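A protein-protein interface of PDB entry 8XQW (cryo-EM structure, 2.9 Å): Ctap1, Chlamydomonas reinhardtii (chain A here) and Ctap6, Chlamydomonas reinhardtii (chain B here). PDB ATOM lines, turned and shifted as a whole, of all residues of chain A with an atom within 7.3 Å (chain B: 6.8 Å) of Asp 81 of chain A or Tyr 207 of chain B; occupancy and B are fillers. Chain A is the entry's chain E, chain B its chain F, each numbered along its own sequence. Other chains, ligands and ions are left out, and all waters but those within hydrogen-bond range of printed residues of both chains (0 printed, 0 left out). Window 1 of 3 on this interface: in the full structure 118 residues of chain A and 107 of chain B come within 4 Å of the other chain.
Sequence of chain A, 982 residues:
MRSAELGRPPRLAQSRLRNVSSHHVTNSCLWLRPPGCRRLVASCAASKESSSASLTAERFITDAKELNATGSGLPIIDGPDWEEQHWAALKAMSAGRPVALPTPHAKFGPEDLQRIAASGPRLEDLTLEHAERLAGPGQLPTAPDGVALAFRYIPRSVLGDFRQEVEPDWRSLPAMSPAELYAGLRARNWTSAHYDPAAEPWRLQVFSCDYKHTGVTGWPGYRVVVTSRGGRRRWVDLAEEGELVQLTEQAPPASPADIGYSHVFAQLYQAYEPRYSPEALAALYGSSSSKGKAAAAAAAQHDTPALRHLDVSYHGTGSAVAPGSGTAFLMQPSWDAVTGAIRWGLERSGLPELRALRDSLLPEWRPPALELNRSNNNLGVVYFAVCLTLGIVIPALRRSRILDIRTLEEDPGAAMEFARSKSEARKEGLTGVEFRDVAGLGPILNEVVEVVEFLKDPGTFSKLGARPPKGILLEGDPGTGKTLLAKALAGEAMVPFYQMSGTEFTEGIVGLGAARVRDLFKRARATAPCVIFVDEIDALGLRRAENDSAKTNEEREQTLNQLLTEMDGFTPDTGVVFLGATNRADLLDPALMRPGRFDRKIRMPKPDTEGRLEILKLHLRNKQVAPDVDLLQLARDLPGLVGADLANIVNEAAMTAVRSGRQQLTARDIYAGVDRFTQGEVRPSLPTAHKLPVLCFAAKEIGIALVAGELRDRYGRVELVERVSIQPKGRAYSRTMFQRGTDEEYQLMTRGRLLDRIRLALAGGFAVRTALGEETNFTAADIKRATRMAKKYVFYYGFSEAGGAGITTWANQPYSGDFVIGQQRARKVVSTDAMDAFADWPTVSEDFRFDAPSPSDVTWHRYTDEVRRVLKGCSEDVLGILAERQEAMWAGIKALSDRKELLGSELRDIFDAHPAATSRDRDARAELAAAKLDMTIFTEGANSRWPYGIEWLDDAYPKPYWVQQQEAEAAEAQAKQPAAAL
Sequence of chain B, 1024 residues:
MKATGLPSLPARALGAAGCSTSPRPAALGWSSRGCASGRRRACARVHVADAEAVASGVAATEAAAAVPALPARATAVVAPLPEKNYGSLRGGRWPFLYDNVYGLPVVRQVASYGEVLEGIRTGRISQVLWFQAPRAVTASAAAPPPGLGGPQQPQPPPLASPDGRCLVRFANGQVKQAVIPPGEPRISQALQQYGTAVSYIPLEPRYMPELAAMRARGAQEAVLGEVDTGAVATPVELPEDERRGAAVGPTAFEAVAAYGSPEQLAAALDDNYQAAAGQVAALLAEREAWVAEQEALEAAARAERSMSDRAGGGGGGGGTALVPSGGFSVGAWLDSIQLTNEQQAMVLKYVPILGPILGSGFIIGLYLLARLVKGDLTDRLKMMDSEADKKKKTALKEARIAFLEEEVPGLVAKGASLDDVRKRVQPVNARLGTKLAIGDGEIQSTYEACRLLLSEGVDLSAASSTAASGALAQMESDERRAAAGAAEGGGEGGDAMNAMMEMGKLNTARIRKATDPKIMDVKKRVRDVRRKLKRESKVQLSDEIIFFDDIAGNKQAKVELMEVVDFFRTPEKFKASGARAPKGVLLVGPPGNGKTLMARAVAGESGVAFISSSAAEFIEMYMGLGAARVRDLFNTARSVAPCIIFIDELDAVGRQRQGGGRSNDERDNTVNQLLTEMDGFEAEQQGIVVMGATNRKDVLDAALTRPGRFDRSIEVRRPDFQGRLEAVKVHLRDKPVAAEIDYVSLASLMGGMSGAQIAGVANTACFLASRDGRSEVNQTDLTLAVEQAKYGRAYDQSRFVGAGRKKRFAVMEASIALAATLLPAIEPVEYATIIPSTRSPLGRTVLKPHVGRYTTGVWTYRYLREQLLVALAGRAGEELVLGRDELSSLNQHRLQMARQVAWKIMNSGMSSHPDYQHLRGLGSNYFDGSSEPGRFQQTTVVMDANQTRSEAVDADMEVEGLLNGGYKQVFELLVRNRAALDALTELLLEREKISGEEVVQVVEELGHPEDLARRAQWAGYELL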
ATOM      1  N   ILE A  76      -5.084  -9.346 -16.488  1.00  0.00           N
ATOM      2  CA  ILE A  76      -6.373  -8.681 -16.335  1.00  0.00           C
ATOM      3  C   ILE A  76      -6.972  -9.132 -15.011  1.00  0.00           C
ATOM      4  O   ILE A  76      -7.463 -10.258 -14.893  1.00  0.00           O
ATOM      5  CB  ILE A  76      -7.307  -8.992 -17.508  1.00  0.00           C
ATOM      6  CG1 ILE A  76      -6.740  -8.410 -18.799  1.00  0.00           C
ATOM      7  CG2 ILE A  76      -8.683  -8.428 -17.247  1.00  0.00           C
ATOM      8  CD1 ILE A  76      -7.392  -8.959 -20.039  1.00  0.00           C
ATOM      9  N   ASP A  78      -9.400  -9.996 -12.332  1.00  0.00           N
ATOM     10  CA  ASP A  78     -10.744 -10.477 -12.603  1.00  0.00           C
ATOM     11  C   ASP A  78     -11.369 -11.010 -11.324  1.00  0.00           C
ATOM     12  O   ASP A  78     -10.692 -11.235 -10.318  1.00  0.00           O
ATOM     13  CB  ASP A  78     -10.731 -11.557 -13.689  1.00  0.00           C
ATOM     14  CG  ASP A  78     -12.088 -11.764 -14.322  1.00  0.00           C
ATOM     15  OD1 ASP A  78     -13.087 -11.868 -13.582  1.00  0.00           O
ATOM     16  OD2 ASP A  78     -12.158 -11.818 -15.566  1.00  0.00           O
ATOM     17  N   GLY A  79     -12.680 -11.206 -11.383  1.00  0.00           N
ATOM     18  CA  GLY A  79     -13.443 -11.726 -10.278  1.00  0.00           C
ATOM     19  C   GLY A  79     -14.922 -11.626 -10.574  1.00  0.00           C
ATOM     20  O   GLY A  79     -15.349 -11.681 -11.730  1.00  0.00           O
ATOM     21  N   PRO A  80     -15.736 -11.482  -9.538  1.00  0.00           N
ATOM     22  CA  PRO A  80     -17.165 -11.253  -9.757  1.00  0.00           C
ATOM     23  C   PRO A  80     -17.425  -9.860 -10.304  1.00  0.00           C
ATOM     24  O   PRO A  80     -16.512  -9.054 -10.486  1.00  0.00           O
ATOM     25  CB  PRO A  80     -17.767 -11.423  -8.359  1.00  0.00           C
ATOM     26  CG  PRO A  80     -16.643 -11.115  -7.434  1.00  0.00           C
ATOM     27  CD  PRO A  80     -15.408 -11.624  -8.111  1.00  0.00           C
ATOM     28  N   ASP A  81     -18.700  -9.582 -10.562  1.00  0.00           N
ATOM     29  CA  ASP A  81     -19.090  -8.298 -11.124  1.00  0.00           C
ATOM     30  C   ASP A  81     -18.988  -7.194 -10.078  1.00  0.00           C
ATOM     31  O   ASP A  81     -18.960  -7.441  -8.874  1.00  0.00           O
ATOM     32  CB  ASP A  81     -20.509  -8.370 -11.672  1.00  0.00           C
ATOM     33  CG  ASP A  81     -20.695  -7.502 -12.891  1.00  0.00           C
ATOM     34  OD1 ASP A  81     -19.696  -6.916 -13.357  1.00  0.00           O
ATOM     35  OD2 ASP A  81     -21.839  -7.395 -13.376  1.00  0.00           O
ATOM     36  N   TRP A  82     -18.954  -5.949 -10.558  1.00  0.00           N
ATOM     37  CA  TRP A  82     -18.587  -4.840  -9.686  1.00  0.00           C
ATOM     38  C   TRP A  82     -19.664  -4.523  -8.663  1.00  0.00           C
ATOM     39  O   TRP A  82     -19.389  -3.859  -7.660  1.00  0.00           O
ATOM     40  CB  TRP A  82     -18.270  -3.599 -10.518  1.00  0.00           C
ATOM     41  CG  TRP A  82     -19.466  -2.917 -11.086  1.00  0.00           C
ATOM     42  CD1 TRP A  82     -20.022  -3.131 -12.310  1.00  0.00           C
ATOM     43  CD2 TRP A  82     -20.252  -1.900 -10.462  1.00  0.00           C
ATOM     44  NE1 TRP A  82     -21.107  -2.315 -12.485  1.00  0.00           N
ATOM     45  CE2 TRP A  82     -21.268  -1.548 -11.363  1.00  0.00           C
ATOM     46  CE3 TRP A  82     -20.196  -1.254  -9.227  1.00  0.00           C
ATOM     47  CZ2 TRP A  82     -22.221  -0.584 -11.067  1.00  0.00           C
ATOM     48  CZ3 TRP A  82     -21.143  -0.298  -8.936  1.00  0.00           C
ATOM     49  CH2 TRP A  82     -22.139   0.029  -9.851  1.00  0.00           C
ATOM     50  N   GLU A  83     -20.888  -4.978  -8.889  1.00  0.00           N
ATOM     51  CA  GLU A  83     -21.996  -4.656  -8.003  1.00  0.00           C
ATOM     52  C   GLU A  83     -22.407  -5.821  -7.120  1.00  0.00           C
ATOM     53  O   GLU A  83     -23.397  -5.708  -6.392  1.00  0.00           O
ATOM     54  CB  GLU A  83     -23.200  -4.192  -8.823  1.00  0.00           C
ATOM     55  CG  GLU A  83     -23.925  -5.320  -9.531  1.00  0.00           C
ATOM     56  CD  GLU A  83     -23.214  -5.778 -10.784  1.00  0.00           C
ATOM     57  OE1 GLU A  83     -21.968  -5.799 -10.790  1.00  0.00           O
ATOM     58  OE2 GLU A  83     -23.898  -6.131 -11.766  1.00  0.00           O
ATOM     59  N   GLU A  84     -21.677  -6.933  -7.162  1.00  0.00           N
ATOM     60  CA  GLU A  84     -22.040  -8.112  -6.388  1.00  0.00           C
ATOM     61  C   GLU A  84     -20.824  -8.764  -5.744  1.00  0.00           C
ATOM     62  O   GLU A  84     -20.907  -9.909  -5.294  1.00  0.00           O
ATOM     63  CB  GLU A  84     -22.770  -9.121  -7.266  1.00  0.00           C
ATOM     64  CG  GLU A  84     -21.886  -9.761  -8.305  1.00  0.00           C
ATOM     65  CD  GLU A  84     -22.635 -10.763  -9.140  1.00  0.00           C
ATOM     66  OE1 GLU A  84     -23.861 -10.892  -8.937  1.00  0.00           O
ATOM     67  OE2 GLU A  84     -22.009 -11.420  -9.998  1.00  0.00           O
ATOM     68  N   GLN A  85     -19.699  -8.057  -5.684  1.00  0.00           N
ATOM     69  CA  GLN A  85     -18.510  -8.621  -5.061  1.00  0.00           C
ATOM     70  C   GLN A  85     -18.724  -8.901  -3.583  1.00  0.00           C
ATOM     71  O   GLN A  85     -18.001  -9.709  -2.993  1.00  0.00           O
ATOM     72  CB  GLN A  85     -17.333  -7.670  -5.233  1.00  0.00           C
ATOM     73  CG  GLN A  85     -16.796  -7.595  -6.629  1.00  0.00           C
ATOM     74  CD  GLN A  85     -15.863  -6.432  -6.800  1.00  0.00           C
ATOM     75  OE1 GLN A  85     -15.711  -5.613  -5.895  1.00  0.00           O
ATOM     76  NE2 GLN A  85     -15.227  -6.344  -7.958  1.00  0.00           N
ATOM     77  N   HIS A  86     -19.702  -8.252  -2.966  1.00  0.00           N
ATOM     78  CA  HIS A  86     -19.842  -8.284  -1.521  1.00  0.00           C
ATOM     79  C   HIS A  86     -20.952  -9.201  -1.042  1.00  0.00           C
ATOM     80  O   HIS A  86     -21.277  -9.180   0.144  1.00  0.00           O
ATOM     81  CB  HIS A  86     -20.084  -6.871  -0.995  1.00  0.00           C
ATOM     82  CG  HIS A  86     -19.043  -5.886  -1.421  1.00  0.00           C
ATOM     83  ND1 HIS A  86     -17.905  -6.252  -2.106  1.00  0.00           N
ATOM     84  CD2 HIS A  86     -18.970  -4.543  -1.267  1.00  0.00           C
ATOM     85  CE1 HIS A  86     -17.175  -5.179  -2.354  1.00  0.00           C
ATOM     86  NE2 HIS A  86     -17.799  -4.128  -1.853  1.00  0.00           N
ATOM     87  N   PRO A 155     -10.927   1.618 -11.164  1.00  0.00           N
ATOM     88  CA  PRO A 155     -11.935   0.581 -11.369  1.00  0.00           C
ATOM     89  C   PRO A 155     -13.238   0.900 -10.652  1.00  0.00           C
ATOM     90  O   PRO A 155     -13.279   1.646  -9.676  1.00  0.00           O
ATOM     91  CB  PRO A 155     -11.273  -0.655 -10.762  1.00  0.00           C
ATOM     92  CG  PRO A 155     -10.473  -0.101  -9.668  1.00  0.00           C
ATOM     93  CD  PRO A 155      -9.965   1.235 -10.122  1.00  0.00           C
ATOM     94  N   ARG A 156     -14.317   0.308 -11.163  1.00  0.00           N
ATOM     95  CA  ARG A 156     -15.627   0.515 -10.561  1.00  0.00           C
ATOM     96  C   ARG A 156     -15.708  -0.056  -9.159  1.00  0.00           C
ATOM     97  O   ARG A 156     -16.561   0.372  -8.377  1.00  0.00           O
ATOM     98  CB  ARG A 156     -16.717  -0.119 -11.419  1.00  0.00           C
ATOM     99  CG  ARG A 156     -16.952   0.556 -12.752  1.00  0.00           C
ATOM    100  CD  ARG A 156     -18.202   1.391 -12.705  1.00  0.00           C
ATOM    101  NE  ARG A 156     -18.849   1.484 -14.004  1.00  0.00           N
ATOM    102  CZ  ARG A 156     -19.968   2.159 -14.219  1.00  0.00           C
ATOM    103  NH1 ARG A 156     -20.559   2.794 -13.221  1.00  0.00           N
ATOM    104  NH2 ARG A 156     -20.500   2.194 -15.427  1.00  0.00           N
ATOM    105  N   SER A 157     -14.845  -1.015  -8.827  1.00  0.00           N
ATOM    106  CA  SER A 157     -14.876  -1.665  -7.525  1.00  0.00           C
ATOM    107  C   SER A 157     -14.576  -0.715  -6.380  1.00  0.00           C
ATOM    108  O   SER A 157     -14.824  -1.069  -5.225  1.00  0.00           O
ATOM    109  CB  SER A 157     -13.885  -2.823  -7.506  1.00  0.00           C
ATOM    110  OG  SER A 157     -13.849  -3.474  -8.763  1.00  0.00           O
ATOM    111  N   VAL B 101     -11.413  -8.062  -5.265  1.00  0.00           N
ATOM    112  CA  VAL B 101     -10.736  -8.305  -6.534  1.00  0.00           C
ATOM    113  C   VAL B 101      -9.455  -7.492  -6.619  1.00  0.00           C
ATOM    114  O   VAL B 101      -8.360  -8.044  -6.769  1.00  0.00           O
ATOM    115  CB  VAL B 101     -11.673  -7.995  -7.710  1.00  0.00           C
ATOM    116  CG1 VAL B 101     -10.961  -8.246  -9.010  1.00  0.00           C
ATOM    117  CG2 VAL B 101     -12.915  -8.837  -7.612  1.00  0.00           C
ATOM    118  N   PRO B 134     -19.793   1.286 -22.271  1.00  0.00           N
ATOM    119  CA  PRO B 134     -19.153   0.940 -23.549  1.00  0.00           C
ATOM    120  C   PRO B 134     -19.814   1.464 -24.822  1.00  0.00           C
ATOM    121  O   PRO B 134     -19.109   1.567 -25.832  1.00  0.00           O
ATOM    122  CB  PRO B 134     -19.155  -0.590 -23.519  1.00  0.00           C
ATOM    123  CG  PRO B 134     -19.118  -0.913 -22.094  1.00  0.00           C
ATOM    124  CD  PRO B 134     -20.029   0.081 -21.467  1.00  0.00           C
ATOM    125  N   LEU B 203     -12.183   3.382 -18.959  1.00  0.00           N
ATOM    126  CA  LEU B 203     -12.784   2.109 -18.607  1.00  0.00           C
ATOM    127  C   LEU B 203     -11.727   1.118 -18.136  1.00  0.00           C
ATOM    128  O   LEU B 203     -10.592   1.116 -18.612  1.00  0.00           O
ATOM    129  CB  LEU B 203     -13.541   1.541 -19.801  1.00  0.00           C
ATOM    130  CG  LEU B 203     -14.982   2.015 -19.921  1.00  0.00           C
ATOM    131  CD1 LEU B 203     -15.434   1.939 -21.347  1.00  0.00           C
ATOM    132  CD2 LEU B 203     -15.866   1.165 -19.049  1.00  0.00           C
ATOM    133  N   GLU B 204     -12.117   0.266 -17.195  1.00  0.00           N
ATOM    134  CA  GLU B 204     -11.143  -0.699 -16.719  1.00  0.00           C
ATOM    135  C   GLU B 204     -11.035  -1.871 -17.687  1.00  0.00           C
ATOM    136  O   GLU B 204     -11.986  -2.172 -18.410  1.00  0.00           O
ATOM    137  CB  GLU B 204     -11.526  -1.208 -15.338  1.00  0.00           C
ATOM    138  CG  GLU B 204     -12.986  -1.478 -15.166  1.00  0.00           C
ATOM    139  CD  GLU B 204     -13.273  -2.203 -13.877  1.00  0.00           C
ATOM    140  OE1 GLU B 204     -12.637  -3.245 -13.633  1.00  0.00           O
ATOM    141  OE2 GLU B 204     -14.126  -1.727 -13.104  1.00  0.00           O
ATOM    142  N   PRO B 205      -9.883  -2.540 -17.711  1.00  0.00           N
ATOM    143  CA  PRO B 205      -9.612  -3.489 -18.798  1.00  0.00           C
ATOM    144  C   PRO B 205     -10.582  -4.646 -18.886  1.00  0.00           C
ATOM    145  O   PRO B 205     -10.882  -5.094 -19.996  1.00  0.00           O
ATOM    146  CB  PRO B 205      -8.193  -3.964 -18.479  1.00  0.00           C
ATOM    147  CG  PRO B 205      -7.597  -2.828 -17.766  1.00  0.00           C
ATOM    148  CD  PRO B 205      -8.682  -2.299 -16.902  1.00  0.00           C
ATOM    149  N   ARG B 206     -11.088  -5.153 -17.770  1.00  0.00           N
ATOM    150  CA  ARG B 206     -12.023  -6.261 -17.888  1.00  0.00           C
ATOM    151  C   ARG B 206     -13.391  -5.819 -18.380  1.00  0.00           C
ATOM    152  O   ARG B 206     -14.298  -6.649 -18.465  1.00  0.00           O
ATOM    153  CB  ARG B 206     -12.164  -6.990 -16.558  1.00  0.00           C
ATOM    154  CG  ARG B 206     -12.796  -6.191 -15.464  1.00  0.00           C
ATOM    155  CD  ARG B 206     -13.389  -7.116 -14.435  1.00  0.00           C
ATOM    156  NE  ARG B 206     -13.651  -6.434 -13.180  1.00  0.00           N
ATOM    157  CZ  ARG B 206     -14.363  -6.956 -12.193  1.00  0.00           C
ATOM    158  NH1 ARG B 206     -14.559  -6.272 -11.076  1.00  0.00           N
ATOM    159  NH2 ARG B 206     -14.881  -8.167 -12.325  1.00  0.00           N
ATOM    160  N   TYR B 207     -13.556  -4.540 -18.708  1.00  0.00           N
ATOM    161  CA  TYR B 207     -14.805  -4.023 -19.233  1.00  0.00           C
ATOM    162  C   TYR B 207     -14.655  -3.327 -20.573  1.00  0.00           C
ATOM    163  O   TYR B 207     -15.669  -3.083 -21.231  1.00  0.00           O
ATOM    164  CB  TYR B 207     -15.439  -3.049 -18.234  1.00  0.00           C
ATOM    165  CG  TYR B 207     -16.107  -3.739 -17.080  1.00  0.00           C
ATOM    166  CD1 TYR B 207     -16.698  -4.974 -17.243  1.00  0.00           C
ATOM    167  CD2 TYR B 207     -16.137  -3.163 -15.829  1.00  0.00           C
ATOM    168  CE1 TYR B 207     -17.309  -5.611 -16.198  1.00  0.00           C
ATOM    169  CE2 TYR B 207     -16.745  -3.794 -14.776  1.00  0.00           C
ATOM    170  CZ  TYR B 207     -17.331  -5.017 -14.968  1.00  0.00           C
ATOM    171  OH  TYR B 207     -17.942  -5.659 -13.922  1.00  0.00           O
ATOM    172  N   MET B 208     -13.442  -2.992 -20.988  1.00  0.00           N
ATOM    173  CA  MET B 208     -13.251  -2.467 -22.328  1.00  0.00           C
ATOM    174  C   MET B 208     -13.653  -3.527 -23.345  1.00  0.00           C
ATOM    175  O   MET B 208     -13.391  -4.715 -23.138  1.00  0.00           O
ATOM    176  CB  MET B 208     -11.797  -2.058 -22.545  1.00  0.00           C
ATOM    177  CG  MET B 208     -11.359  -0.908 -21.677  1.00  0.00           C
ATOM    178  SD  MET B 208      -9.667  -0.406 -22.001  1.00  0.00           S
ATOM    179  CE  MET B 208      -9.810   0.139 -23.691  1.00  0.00           C
ATOM    180  N   PRO B 209     -14.300  -3.143 -24.447  1.00  0.00           N
ATOM    181  CA  PRO B 209     -14.766  -4.144 -25.412  1.00  0.00           C
ATOM    182  C   PRO B 209     -13.676  -4.681 -26.316  1.00  0.00           C
ATOM    183  O   PRO B 209     -13.883  -5.731 -26.936  1.00  0.00           O
ATOM    184  CB  PRO B 209     -15.816  -3.382 -26.228  1.00  0.00           C
ATOM    185  CG  PRO B 209     -16.008  -2.078 -25.526  1.00  0.00           C
ATOM    186  CD  PRO B 209     -14.741  -1.795 -24.816  1.00  0.00           C
ATOM    187  N   GLU B 210     -12.535  -4.009 -26.421  1.00  0.00           N
ATOM    188  CA  GLU B 210     -11.469  -4.467 -27.296  1.00  0.00           C
ATOM    189  C   GLU B 210     -10.563  -5.504 -26.651  1.00  0.00           C
ATOM    190  O   GLU B 210      -9.798  -6.159 -27.363  1.00  0.00           O
ATOM    191  CB  GLU B 210     -10.620  -3.286 -27.752  1.00  0.00           C
ATOM    192  CG  GLU B 210     -11.426  -2.112 -28.232  1.00  0.00           C
ATOM    193  CD  GLU B 210     -10.840  -0.803 -27.772  1.00  0.00           C
ATOM    194  OE1 GLU B 210     -11.022   0.215 -28.467  1.00  0.00           O
ATOM    195  OE2 GLU B 210     -10.189  -0.797 -26.708  1.00  0.00           O
ATOM    196  N   LEU B 211     -10.627  -5.669 -25.335  1.00  0.00           N
ATOM    197  CA  LEU B 211      -9.790  -6.636 -24.637  1.00  0.00           C
ATOM    198  C   LEU B 211     -10.599  -7.801 -24.090  1.00  0.00           C
ATOM    199  O   LEU B 211     -10.119  -8.525 -23.217  1.00  0.00           O
ATOM    200  CB  LEU B 211      -9.013  -5.957 -23.513  1.00  0.00           C
ATOM    201  CG  LEU B 211      -8.332  -4.659 -23.924  1.00  0.00           C
ATOM    202  CD1 LEU B 211      -7.609  -4.055 -22.748  1.00  0.00           C
ATOM    203  CD2 LEU B 211      -7.379  -4.904 -25.072  1.00  0.00           C
ATOM    204  N   ALA B 212     -11.823  -7.995 -24.577  1.00  0.00           N
ATOM    205  CA  ALA B 212     -12.593  -9.156 -24.153  1.00  0.00           C
ATOM    206  C   ALA B 212     -11.945 -10.449 -24.619  1.00  0.00           C
ATOM    207  O   ALA B 212     -12.073 -11.483 -23.955  1.00  0.00           O
ATOM    208  CB  ALA B 212     -14.021  -9.061 -24.677  1.00  0.00           C
ATOM    209  N   ARG B 215      -9.347 -11.123 -21.990  1.00  0.00           N
ATOM    210  CA  ARG B 215      -9.999 -11.580 -20.771  1.00  0.00           C
ATOM    211  C   ARG B 215     -10.425 -13.036 -20.900  1.00  0.00           C
ATOM    212  O   ARG B 215     -10.211 -13.845 -19.989  1.00  0.00           O
ATOM    213  CB  ARG B 215     -11.198 -10.688 -20.461  1.00  0.00           C
ATOM    214  CG  ARG B 215     -11.921 -11.031 -19.181  1.00  0.00           C
ATOM    215  CD  ARG B 215     -13.225 -10.270 -19.081  1.00  0.00           C
ATOM    216  NE  ARG B 215     -13.909 -10.528 -17.820  1.00  0.00           N
ATOM    217  CZ  ARG B 215     -15.097 -10.030 -17.497  1.00  0.00           C
ATOM    218  NH1 ARG B 215     -15.645 -10.325 -16.325  1.00  0.00           N
ATOM    219  NH2 ARG B 215     -15.740  -9.236 -18.340  1.00  0.00           N
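The backbone NH of Arg 156 of chain A is in hydrogen-bond range of the side-chain carboxylate of Glu 204 of chain B, at 2.8 Å. The guanidinium group (NE) of Arg 215 of chain B lies within salt-bridge range of the side-chain carboxylate (OD2) of Asp 78 of chain A. NH2 of Arg 206 of chain B lies within hydrogen-bond range of O of Pro 80 of chain A, 2.6 Å away. The side-chain carboxylate (OD1) of Asp 81 of chain A lies close to the side-chain hydroxyl (OH) of Tyr 207 of chain B, 2.2 Å away. The side-chain amide nitrogen (NE2) of Gln 85 of chain A sits close to the guanidinium group (NH1) of Arg 206 of chain B (3.2 Å).
Of the printed residues of chain B, Gly 79 of chain A touches Val 101 (3.97 Å) and Arg 206 (3.6 Å). Of the printed residues of chain B, Pro 80 of chain A touches Val 101 and Arg 206. Asp 81 of chain A touches just one residue of chain B: Tyr 207 (2.2 Å). Printed residues of chain A within 4 Å of Glu 204 of chain B: Pro 155 and Arg 156. Leu 211 of chain B touches none of the printed residues of chain A. The nearest residue of chain A that does not touch Tyr 207 of chain B is Arg 156 of chain A (4.8 Å). The nearest printed residue of chain A that does not touch Arg 215 of chain B is Gly 79 of chain A (4.8 Å).
Of the 13 printed residues of chain B, 5 touch a printed residue of chain A. Hydrophobic or aromatic side chains of chain B that line the printed part of chain A: Val 101 and Tyr 207. Hydrophobic or aromatic side chains of chain A that line the printed part of chain B: Ile 76, Pro 80, Trp 82 and Pro 155.
The backbone carbonyl oxygen of Arg 206 of chain B sits at hydrogen-bond distance from the guanidinium group of Arg 215 of chain B (3.0 Å). OG of Ser 157 of chain A lies within hydrogen-bond range of NE2 of Gln 85 of chain A. OE1 of Glu 204 of chain B is in salt-bridge range of NE of Arg 206 of chain B, at 3.4 Å.
Among the printed residues, pairs that only touch across the chains: Ile 76 of chain A with Arg 206 of chain B, Ile 76 of chain A with Arg 215 of chain B, Asp 78 of chain A with Val 101 of chain B, Gly 79 of chain A with Val 101 of chain B, Gly 79 of chain A with Arg 206 of chain B, Pro 80 of chain A with Val 101 of chain B, Trp 82 of chain A with Tyr 207 of chain B, Gln 85 of chain A with Val 101 of chain B, Pro 155 of chain A with Glu 204 of chain B and Ser 157 of chain A with Arg 206 of chain B.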
